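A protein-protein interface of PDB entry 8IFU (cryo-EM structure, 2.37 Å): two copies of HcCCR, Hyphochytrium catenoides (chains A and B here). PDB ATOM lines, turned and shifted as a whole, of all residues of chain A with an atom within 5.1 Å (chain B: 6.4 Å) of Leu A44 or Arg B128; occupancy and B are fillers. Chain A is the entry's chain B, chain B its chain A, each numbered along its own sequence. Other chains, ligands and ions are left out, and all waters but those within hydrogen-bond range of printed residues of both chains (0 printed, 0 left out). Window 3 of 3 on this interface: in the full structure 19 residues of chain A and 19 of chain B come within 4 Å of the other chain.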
ATOM      1  N   GLY A  40     -16.756 -24.254  24.141  1.00  0.00           N
ATOM      2  CA  GLY A  40     -18.164 -24.007  24.328  1.00  0.00           C
ATOM      3  C   GLY A  40     -18.432 -23.044  25.441  1.00  0.00           C
ATOM      4  O   GLY A  40     -19.423 -22.343  25.417  1.00  0.00           O
ATOM      5  N   ALA A  41     -17.548 -22.984  26.421  1.00  0.00           N
ATOM      6  CA  ALA A  41     -17.680 -22.051  27.517  1.00  0.00           C
ATOM      7  C   ALA A  41     -17.270 -20.667  27.113  1.00  0.00           C
ATOM      8  O   ALA A  41     -17.853 -19.710  27.580  1.00  0.00           O
ATOM      9  CB  ALA A  41     -16.861 -22.518  28.687  1.00  0.00           C
ATOM     10  N   TRP A  42     -16.277 -20.533  26.249  1.00  0.00           N
ATOM     11  CA  TRP A  42     -15.930 -19.228  25.748  1.00  0.00           C
ATOM     12  C   TRP A  42     -17.031 -18.746  24.844  1.00  0.00           C
ATOM     13  O   TRP A  42     -17.353 -17.576  24.827  1.00  0.00           O
ATOM     14  CB  TRP A  42     -14.610 -19.238  24.992  1.00  0.00           C
ATOM     15  CG  TRP A  42     -14.291 -17.890  24.421  1.00  0.00           C
ATOM     16  CD1 TRP A  42     -13.718 -16.847  25.072  1.00  0.00           C
ATOM     17  CD2 TRP A  42     -14.573 -17.426  23.093  1.00  0.00           C
ATOM     18  NE1 TRP A  42     -13.612 -15.768  24.238  1.00  0.00           N
ATOM     19  CE2 TRP A  42     -14.135 -16.098  23.017  1.00  0.00           C
ATOM     20  CE3 TRP A  42     -15.158 -18.008  21.966  1.00  0.00           C
ATOM     21  CZ2 TRP A  42     -14.245 -15.347  21.857  1.00  0.00           C
ATOM     22  CZ3 TRP A  42     -15.277 -17.258  20.829  1.00  0.00           C
ATOM     23  CH2 TRP A  42     -14.821 -15.945  20.776  1.00  0.00           C
ATOM     24  N   MET A  43     -17.616 -19.642  24.077  1.00  0.00           N
ATOM     25  CA  MET A  43     -18.684 -19.282  23.191  1.00  0.00           C
ATOM     26  C   MET A  43     -19.879 -18.769  23.952  1.00  0.00           C
ATOM     27  O   MET A  43     -20.482 -17.802  23.543  1.00  0.00           O
ATOM     28  CB  MET A  43     -19.062 -20.479  22.367  1.00  0.00           C
ATOM     29  CG  MET A  43     -18.869 -20.303  20.884  1.00  0.00           C
ATOM     30  SD  MET A  43     -17.776 -21.514  20.139  1.00  0.00           S
ATOM     31  CE  MET A  43     -18.611 -23.035  20.497  1.00  0.00           C
ATOM     32  N   LEU A  44     -20.225 -19.396  25.058  1.00  0.00           N
ATOM     33  CA  LEU A  44     -21.318 -18.936  25.885  1.00  0.00           C
ATOM     34  C   LEU A  44     -21.015 -17.583  26.459  1.00  0.00           C
ATOM     35  O   LEU A  44     -21.868 -16.716  26.458  1.00  0.00           O
ATOM     36  CB  LEU A  44     -21.548 -19.926  27.012  1.00  0.00           C
ATOM     37  CG  LEU A  44     -22.757 -20.850  26.939  1.00  0.00           C
ATOM     38  CD1 LEU A  44     -23.217 -21.194  28.343  1.00  0.00           C
ATOM     39  CD2 LEU A  44     -23.882 -20.213  26.146  1.00  0.00           C
ATOM     40  N   TYR A  45     -19.809 -17.390  26.961  1.00  0.00           N
ATOM     41  CA  TYR A  45     -19.392 -16.116  27.466  1.00  0.00           C
ATOM     42  C   TYR A  45     -19.526 -15.039  26.423  1.00  0.00           C
ATOM     43  O   TYR A  45     -20.056 -13.974  26.701  1.00  0.00           O
ATOM     44  CB  TYR A  45     -17.947 -16.251  27.936  1.00  0.00           C
ATOM     45  CG  TYR A  45     -17.152 -14.978  28.050  1.00  0.00           C
ATOM     46  CD1 TYR A  45     -17.289 -14.155  29.152  1.00  0.00           C
ATOM     47  CD2 TYR A  45     -16.239 -14.615  27.070  1.00  0.00           C
ATOM     48  CE1 TYR A  45     -16.561 -12.994  29.265  1.00  0.00           C
ATOM     49  CE2 TYR A  45     -15.514 -13.455  27.172  1.00  0.00           C
ATOM     50  CZ  TYR A  45     -15.676 -12.651  28.273  1.00  0.00           C
ATOM     51  OH  TYR A  45     -14.952 -11.492  28.389  1.00  0.00           O
ATOM     52  N   ARG A  46     -19.056 -15.293  25.218  1.00  0.00           N
ATOM     53  CA  ARG A  46     -19.070 -14.287  24.189  1.00  0.00           C
ATOM     54  C   ARG A  46     -20.446 -13.979  23.663  1.00  0.00           C
ATOM     55  O   ARG A  46     -20.681 -12.887  23.166  1.00  0.00           O
ATOM     56  CB  ARG A  46     -18.131 -14.680  23.078  1.00  0.00           C
ATOM     57  CG  ARG A  46     -17.231 -13.543  22.661  1.00  0.00           C
ATOM     58  CD  ARG A  46     -17.723 -12.990  21.349  1.00  0.00           C
ATOM     59  NE  ARG A  46     -17.220 -11.657  21.063  1.00  0.00           N
ATOM     60  CZ  ARG A  46     -17.962 -10.559  21.079  1.00  0.00           C
ATOM     61  NH1 ARG A  46     -17.412  -9.402  20.773  1.00  0.00           N
ATOM     62  NH2 ARG A  46     -19.245 -10.619  21.396  1.00  0.00           N
ATOM     63  N   LEU A  47     -21.368 -14.920  23.770  1.00  0.00           N
ATOM     64  CA  LEU A  47     -22.723 -14.681  23.368  1.00  0.00           C
ATOM     65  C   LEU A  47     -23.288 -13.636  24.260  1.00  0.00           C
ATOM     66  O   LEU A  47     -23.848 -12.663  23.799  1.00  0.00           O
ATOM     67  CB  LEU A  47     -23.527 -15.944  23.568  1.00  0.00           C
ATOM     68  CG  LEU A  47     -23.642 -16.875  22.382  1.00  0.00           C
ATOM     69  CD1 LEU A  47     -24.263 -18.169  22.858  1.00  0.00           C
ATOM     70  CD2 LEU A  47     -24.487 -16.205  21.319  1.00  0.00           C
ATOM     71  N   ASP A  48     -23.139 -13.821  25.551  1.00  0.00           N
ATOM     72  CA  ASP A  48     -23.692 -12.906  26.514  1.00  0.00           C
ATOM     73  C   ASP A  48     -23.025 -11.554  26.581  1.00  0.00           C
ATOM     74  O   ASP A  48     -23.568 -10.639  27.177  1.00  0.00           O
ATOM     75  CB  ASP A  48     -23.605 -13.571  27.866  1.00  0.00           C
ATOM     76  CG  ASP A  48     -24.338 -14.887  27.916  1.00  0.00           C
ATOM     77  OD1 ASP A  48     -25.390 -15.011  27.257  1.00  0.00           O
ATOM     78  OD2 ASP A  48     -23.861 -15.799  28.617  1.00  0.00           O
ATOM     79  N   ALA A  63     -29.299 -12.882  25.196  1.00  0.00           N
ATOM     80  CA  ALA A  63     -28.995 -13.399  23.880  1.00  0.00           C
ATOM     81  C   ALA A  63     -30.132 -14.187  23.322  1.00  0.00           C
ATOM     82  O   ALA A  63     -30.839 -14.841  24.065  1.00  0.00           O
ATOM     83  CB  ALA A  63     -27.744 -14.256  23.954  1.00  0.00           C
ATOM     84  N   SER A  68     -27.316 -20.085  20.731  1.00  0.00           N
ATOM     85  CA  SER A  68     -26.530 -20.890  21.652  1.00  0.00           C
ATOM     86  C   SER A  68     -26.196 -22.301  21.240  1.00  0.00           C
ATOM     87  O   SER A  68     -25.536 -22.983  21.982  1.00  0.00           O
ATOM     88  CB  SER A  68     -27.261 -20.946  22.981  1.00  0.00           C
ATOM     89  OG  SER A  68     -28.255 -19.948  23.054  1.00  0.00           O
ATOM     90  N   ALA A  71     -22.344 -23.254  21.110  1.00  0.00           N
ATOM     91  CA  ALA A  71     -21.813 -23.419  22.440  1.00  0.00           C
ATOM     92  C   ALA A  71     -22.271 -24.675  23.078  1.00  0.00           C
ATOM     93  O   ALA A  71     -21.484 -25.370  23.670  1.00  0.00           O
ATOM     94  CB  ALA A  71     -22.241 -22.256  23.271  1.00  0.00           C
ATOM     95  N   LEU A  72     -23.545 -24.993  22.938  1.00  0.00           N
ATOM     96  CA  LEU A  72     -24.102 -26.171  23.541  1.00  0.00           C
ATOM     97  C   LEU A  72     -23.602 -27.464  22.948  1.00  0.00           C
ATOM     98  O   LEU A  72     -23.405 -28.412  23.660  1.00  0.00           O
ATOM     99  CB  LEU A  72     -25.619 -26.115  23.474  1.00  0.00           C
ATOM    100  CG  LEU A  72     -26.334 -25.151  24.413  1.00  0.00           C
ATOM    101  CD1 LEU A  72     -27.830 -25.178  24.148  1.00  0.00           C
ATOM    102  CD2 LEU A  72     -26.027 -25.460  25.866  1.00  0.00           C
ATOM    103  N   LEU A  75     -20.140 -27.858  24.453  1.00  0.00           N
ATOM    104  CA  LEU A  75     -20.191 -28.168  25.863  1.00  0.00           C
ATOM    105  C   LEU A  75     -20.704 -29.562  26.116  1.00  0.00           C
ATOM    106  O   LEU A  75     -20.244 -30.213  27.030  1.00  0.00           O
ATOM    107  CB  LEU A  75     -21.059 -27.155  26.577  1.00  0.00           C
ATOM    108  CG  LEU A  75     -20.483 -25.794  26.936  1.00  0.00           C
ATOM    109  CD1 LEU A  75     -21.614 -24.822  27.203  1.00  0.00           C
ATOM    110  CD2 LEU A  75     -19.567 -25.897  28.136  1.00  0.00           C
ATOM    111  N   HIS B 125     -32.659 -17.762  28.731  1.00  0.00           N
ATOM    112  CA  HIS B 125     -31.781 -18.929  28.585  1.00  0.00           C
ATOM    113  C   HIS B 125     -32.424 -20.233  28.928  1.00  0.00           C
ATOM    114  O   HIS B 125     -31.792 -21.089  29.498  1.00  0.00           O
ATOM    115  CB  HIS B 125     -30.462 -18.773  29.336  1.00  0.00           C
ATOM    116  CG  HIS B 125     -29.883 -17.397  29.279  1.00  0.00           C
ATOM    117  ND1 HIS B 125     -29.772 -16.680  28.108  1.00  0.00           N
ATOM    118  CD2 HIS B 125     -29.374 -16.610  30.252  1.00  0.00           C
ATOM    119  CE1 HIS B 125     -29.227 -15.507  28.365  1.00  0.00           C
ATOM    120  NE2 HIS B 125     -28.974 -15.440  29.658  1.00  0.00           N
ATOM    121  N   LYS B 126     -33.669 -20.413  28.530  1.00  0.00           N
ATOM    122  CA  LYS B 126     -34.389 -21.628  28.833  1.00  0.00           C
ATOM    123  C   LYS B 126     -33.716 -22.877  28.299  1.00  0.00           C
ATOM    124  O   LYS B 126     -33.659 -23.866  28.992  1.00  0.00           O
ATOM    125  CB  LYS B 126     -35.826 -21.526  28.335  1.00  0.00           C
ATOM    126  CG  LYS B 126     -36.651 -20.482  29.050  1.00  0.00           C
ATOM    127  CD  LYS B 126     -38.119 -20.629  28.721  1.00  0.00           C
ATOM    128  CE  LYS B 126     -38.935 -19.484  29.284  1.00  0.00           C
ATOM    129  NZ  LYS B 126     -38.446 -18.152  28.855  1.00  0.00           N
ATOM    130  N   LEU B 127     -33.188 -22.835  27.088  1.00  0.00           N
ATOM    131  CA  LEU B 127     -32.496 -23.975  26.508  1.00  0.00           C
ATOM    132  C   LEU B 127     -31.246 -24.323  27.251  1.00  0.00           C
ATOM    133  O   LEU B 127     -30.988 -25.476  27.495  1.00  0.00           O
ATOM    134  CB  LEU B 127     -32.136 -23.689  25.060  1.00  0.00           C
ATOM    135  CG  LEU B 127     -32.796 -24.488  23.942  1.00  0.00           C
ATOM    136  CD1 LEU B 127     -31.737 -24.936  22.952  1.00  0.00           C
ATOM    137  CD2 LEU B 127     -33.570 -25.676  24.486  1.00  0.00           C
ATOM    138  N   ARG B 128     -30.472 -23.331  27.633  1.00  0.00           N
ATOM    139  CA  ARG B 128     -29.261 -23.553  28.370  1.00  0.00           C
ATOM    140  C   ARG B 128     -29.536 -24.178  29.699  1.00  0.00           C
ATOM    141  O   ARG B 128     -28.812 -25.054  30.120  1.00  0.00           O
ATOM    142  CB  ARG B 128     -28.569 -22.229  28.601  1.00  0.00           C
ATOM    143  CG  ARG B 128     -28.147 -21.479  27.365  1.00  0.00           C
ATOM    144  CD  ARG B 128     -27.125 -20.449  27.788  1.00  0.00           C
ATOM    145  NE  ARG B 128     -27.118 -19.268  26.944  1.00  0.00           N
ATOM    146  CZ  ARG B 128     -26.565 -18.120  27.303  1.00  0.00           C
ATOM    147  NH1 ARG B 128     -25.995 -18.010  28.491  1.00  0.00           N
ATOM    148  NH2 ARG B 128     -26.586 -17.085  26.481  1.00  0.00           N
ATOM    149  N   PHE B 129     -30.590 -23.740  30.365  1.00  0.00           N
ATOM    150  CA  PHE B 129     -30.950 -24.280  31.661  1.00  0.00           C
ATOM    151  C   PHE B 129     -31.471 -25.698  31.608  1.00  0.00           C
ATOM    152  O   PHE B 129     -31.139 -26.501  32.455  1.00  0.00           O
ATOM    153  CB  PHE B 129     -31.926 -23.343  32.373  1.00  0.00           C
ATOM    154  CG  PHE B 129     -31.278 -22.126  32.953  1.00  0.00           C
ATOM    155  CD1 PHE B 129     -30.205 -22.242  33.809  1.00  0.00           C
ATOM    156  CD2 PHE B 129     -31.740 -20.867  32.641  1.00  0.00           C
ATOM    157  CE1 PHE B 129     -29.608 -21.126  34.347  1.00  0.00           C
ATOM    158  CE2 PHE B 129     -31.140 -19.747  33.163  1.00  0.00           C
ATOM    159  CZ  PHE B 129     -30.078 -19.875  34.023  1.00  0.00           C
ATOM    160  N   VAL B 130     -32.266 -26.019  30.606  1.00  0.00           N
ATOM    161  CA  VAL B 130     -32.813 -27.358  30.479  1.00  0.00           C
ATOM    162  C   VAL B 130     -31.722 -28.314  30.101  1.00  0.00           C
ATOM    163  O   VAL B 130     -31.591 -29.359  30.701  1.00  0.00           O
ATOM    164  CB  VAL B 130     -34.012 -27.412  29.510  1.00  0.00           C
ATOM    165  CG1 VAL B 130     -34.519 -28.830  29.338  1.00  0.00           C
ATOM    166  CG2 VAL B 130     -35.145 -26.567  30.043  1.00  0.00           C
ATOM    167  N   PHE B 131     -30.897 -27.942  29.135  1.00  0.00           N
ATOM    168  CA  PHE B 131     -29.771 -28.768  28.748  1.00  0.00           C
ATOM    169  C   PHE B 131     -28.897 -29.025  29.942  1.00  0.00           C
ATOM    170  O   PHE B 131     -28.554 -30.149  30.186  1.00  0.00           O
ATOM    171  CB  PHE B 131     -28.960 -28.085  27.660  1.00  0.00           C
ATOM    172  CG  PHE B 131     -29.322 -28.506  26.274  1.00  0.00           C
ATOM    173  CD1 PHE B 131     -30.528 -28.133  25.713  1.00  0.00           C
ATOM    174  CD2 PHE B 131     -28.451 -29.265  25.524  1.00  0.00           C
ATOM    175  CE1 PHE B 131     -30.864 -28.514  24.434  1.00  0.00           C
ATOM    176  CE2 PHE B 131     -28.778 -29.650  24.244  1.00  0.00           C
ATOM    177  CZ  PHE B 131     -29.988 -29.275  23.697  1.00  0.00           C
ATOM    178  N   ALA B 132     -28.558 -27.994  30.700  1.00  0.00           N
ATOM    179  CA  ALA B 132     -27.768 -28.160  31.902  1.00  0.00           C
ATOM    180  C   ALA B 132     -28.298 -29.202  32.828  1.00  0.00           C
ATOM    181  O   ALA B 132     -27.586 -30.101  33.165  1.00  0.00           O
ATOM    182  CB  ALA B 132     -27.605 -26.849  32.635  1.00  0.00           C
ATOM    183  N   VAL B 133     -29.559 -29.113  33.209  1.00  0.00           N
ATOM    184  CA  VAL B 133     -30.173 -30.096  34.087  1.00  0.00           C
ATOM    185  C   VAL B 133     -30.189 -31.522  33.544  1.00  0.00           C
ATOM    186  O   VAL B 133     -30.012 -32.454  34.289  1.00  0.00           O
ATOM    187  CB  VAL B 133     -31.541 -29.611  34.635  1.00  0.00           C
ATOM    188  CG1 VAL B 133     -32.729 -30.107  33.825  1.00  0.00           C
ATOM    189  CG2 VAL B 133     -31.691 -29.977  36.101  1.00  0.00           C
ATOM    190  N   TRP B 161     -21.674 -28.770  36.251  1.00  0.00           N
ATOM    191  CA  TRP B 161     -22.784 -28.299  35.460  1.00  0.00           C
ATOM    192  C   TRP B 161     -23.868 -27.723  36.333  1.00  0.00           C
ATOM    193  O   TRP B 161     -24.591 -26.849  35.898  1.00  0.00           O
ATOM    194  CB  TRP B 161     -23.351 -29.442  34.645  1.00  0.00           C
ATOM    195  CG  TRP B 161     -22.701 -29.624  33.337  1.00  0.00           C
ATOM    196  CD1 TRP B 161     -21.637 -30.418  33.058  1.00  0.00           C
ATOM    197  CD2 TRP B 161     -23.066 -28.993  32.112  1.00  0.00           C
ATOM    198  NE1 TRP B 161     -21.312 -30.321  31.736  1.00  0.00           N
ATOM    199  CE2 TRP B 161     -22.176 -29.451  31.129  1.00  0.00           C
ATOM    200  CE3 TRP B 161     -24.060 -28.083  31.751  1.00  0.00           C
ATOM    201  CZ2 TRP B 161     -22.248 -29.031  29.810  1.00  0.00           C
ATOM    202  CZ3 TRP B 161     -24.133 -27.672  30.443  1.00  0.00           C
ATOM    203  CH2 TRP B 161     -23.232 -28.143  29.486  1.00  0.00           C
ATOM    204  N   PHE B 165     -25.306 -23.575  36.819  1.00  0.00           N
ATOM    205  CA  PHE B 165     -26.755 -23.539  36.632  1.00  0.00           C
ATOM    206  C   PHE B 165     -27.505 -22.923  37.792  1.00  0.00           C
ATOM    207  O   PHE B 165     -28.316 -22.037  37.599  1.00  0.00           O
ATOM    208  CB  PHE B 165     -27.179 -25.001  36.433  1.00  0.00           C
ATOM    209  CG  PHE B 165     -28.649 -25.296  36.569  1.00  0.00           C
ATOM    210  CD1 PHE B 165     -29.475 -25.246  35.472  1.00  0.00           C
ATOM    211  CD2 PHE B 165     -29.177 -25.744  37.769  1.00  0.00           C
ATOM    212  CE1 PHE B 165     -30.812 -25.559  35.584  1.00  0.00           C
ATOM    213  CE2 PHE B 165     -30.514 -26.044  37.891  1.00  0.00           C
ATOM    214  CZ  PHE B 165     -31.330 -25.962  36.791  1.00  0.00           C
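Printed residues of chain A that touch a printed residue of chain B: Leu A44, Asp A48, Ala A63 and Leu A75.
Hydrophobic or aromatic side chains of chain A within 4 Å of the printed part of chain B: Leu A44, Ala A63 and Leu A75.
Of the 11 printed residues of chain B, 2 touch a printed residue of chain A.
Printed residues of chain B that touch a printed residue of chain A: Arg B128 and Trp B161.
Hydrophobic or aromatic side chains of chain B within 4 Å of the printed part of chain A: Trp B161.
Along chain B the printed residues that touch a printed residue of chain A span positions 128 to 161.
No position is printed for both chains.
Among the printed residues, merely in contact across the chains: Leu A44 with Arg B128, Leu A75 with Trp B161 and Ala A63 with Arg B128.
The guanidinium group (NH2) of Arg B128 is in salt-bridge range of the side-chain carboxylate (OD1) of Asp A48 (2.5 Å).
Of the printed residues of chain B, Leu A44 touches Arg B128 (3.5 Å).
Of the printed residues of chain B, Asp A48 touches Arg B128.
Of the printed residues of chain B, Ala A63 touches Arg B128 (3.97 Å).
Of the printed residues of chain B, Leu A75 touches Trp B161.
Arg B128 touches just these residues of chain A: Leu A44 (3.5 Å), Asp A48 (2.5 Å) and Ala A63 (3.97 Å).
Of the printed residues of chain A, Trp B161 touches Leu A75.
Phe B165 touches none of the printed residues of chain A.
The nearest printed residue of chain B that does not touch Leu A44 is Trp B161 (6.9 Å).
The nearest residue of chain A that does not touch Arg B128 is Ser A68 (4.1 Å).
The nearest printed residue of chain B that does not touch Asp A48 is His B125 (4.02 Å).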
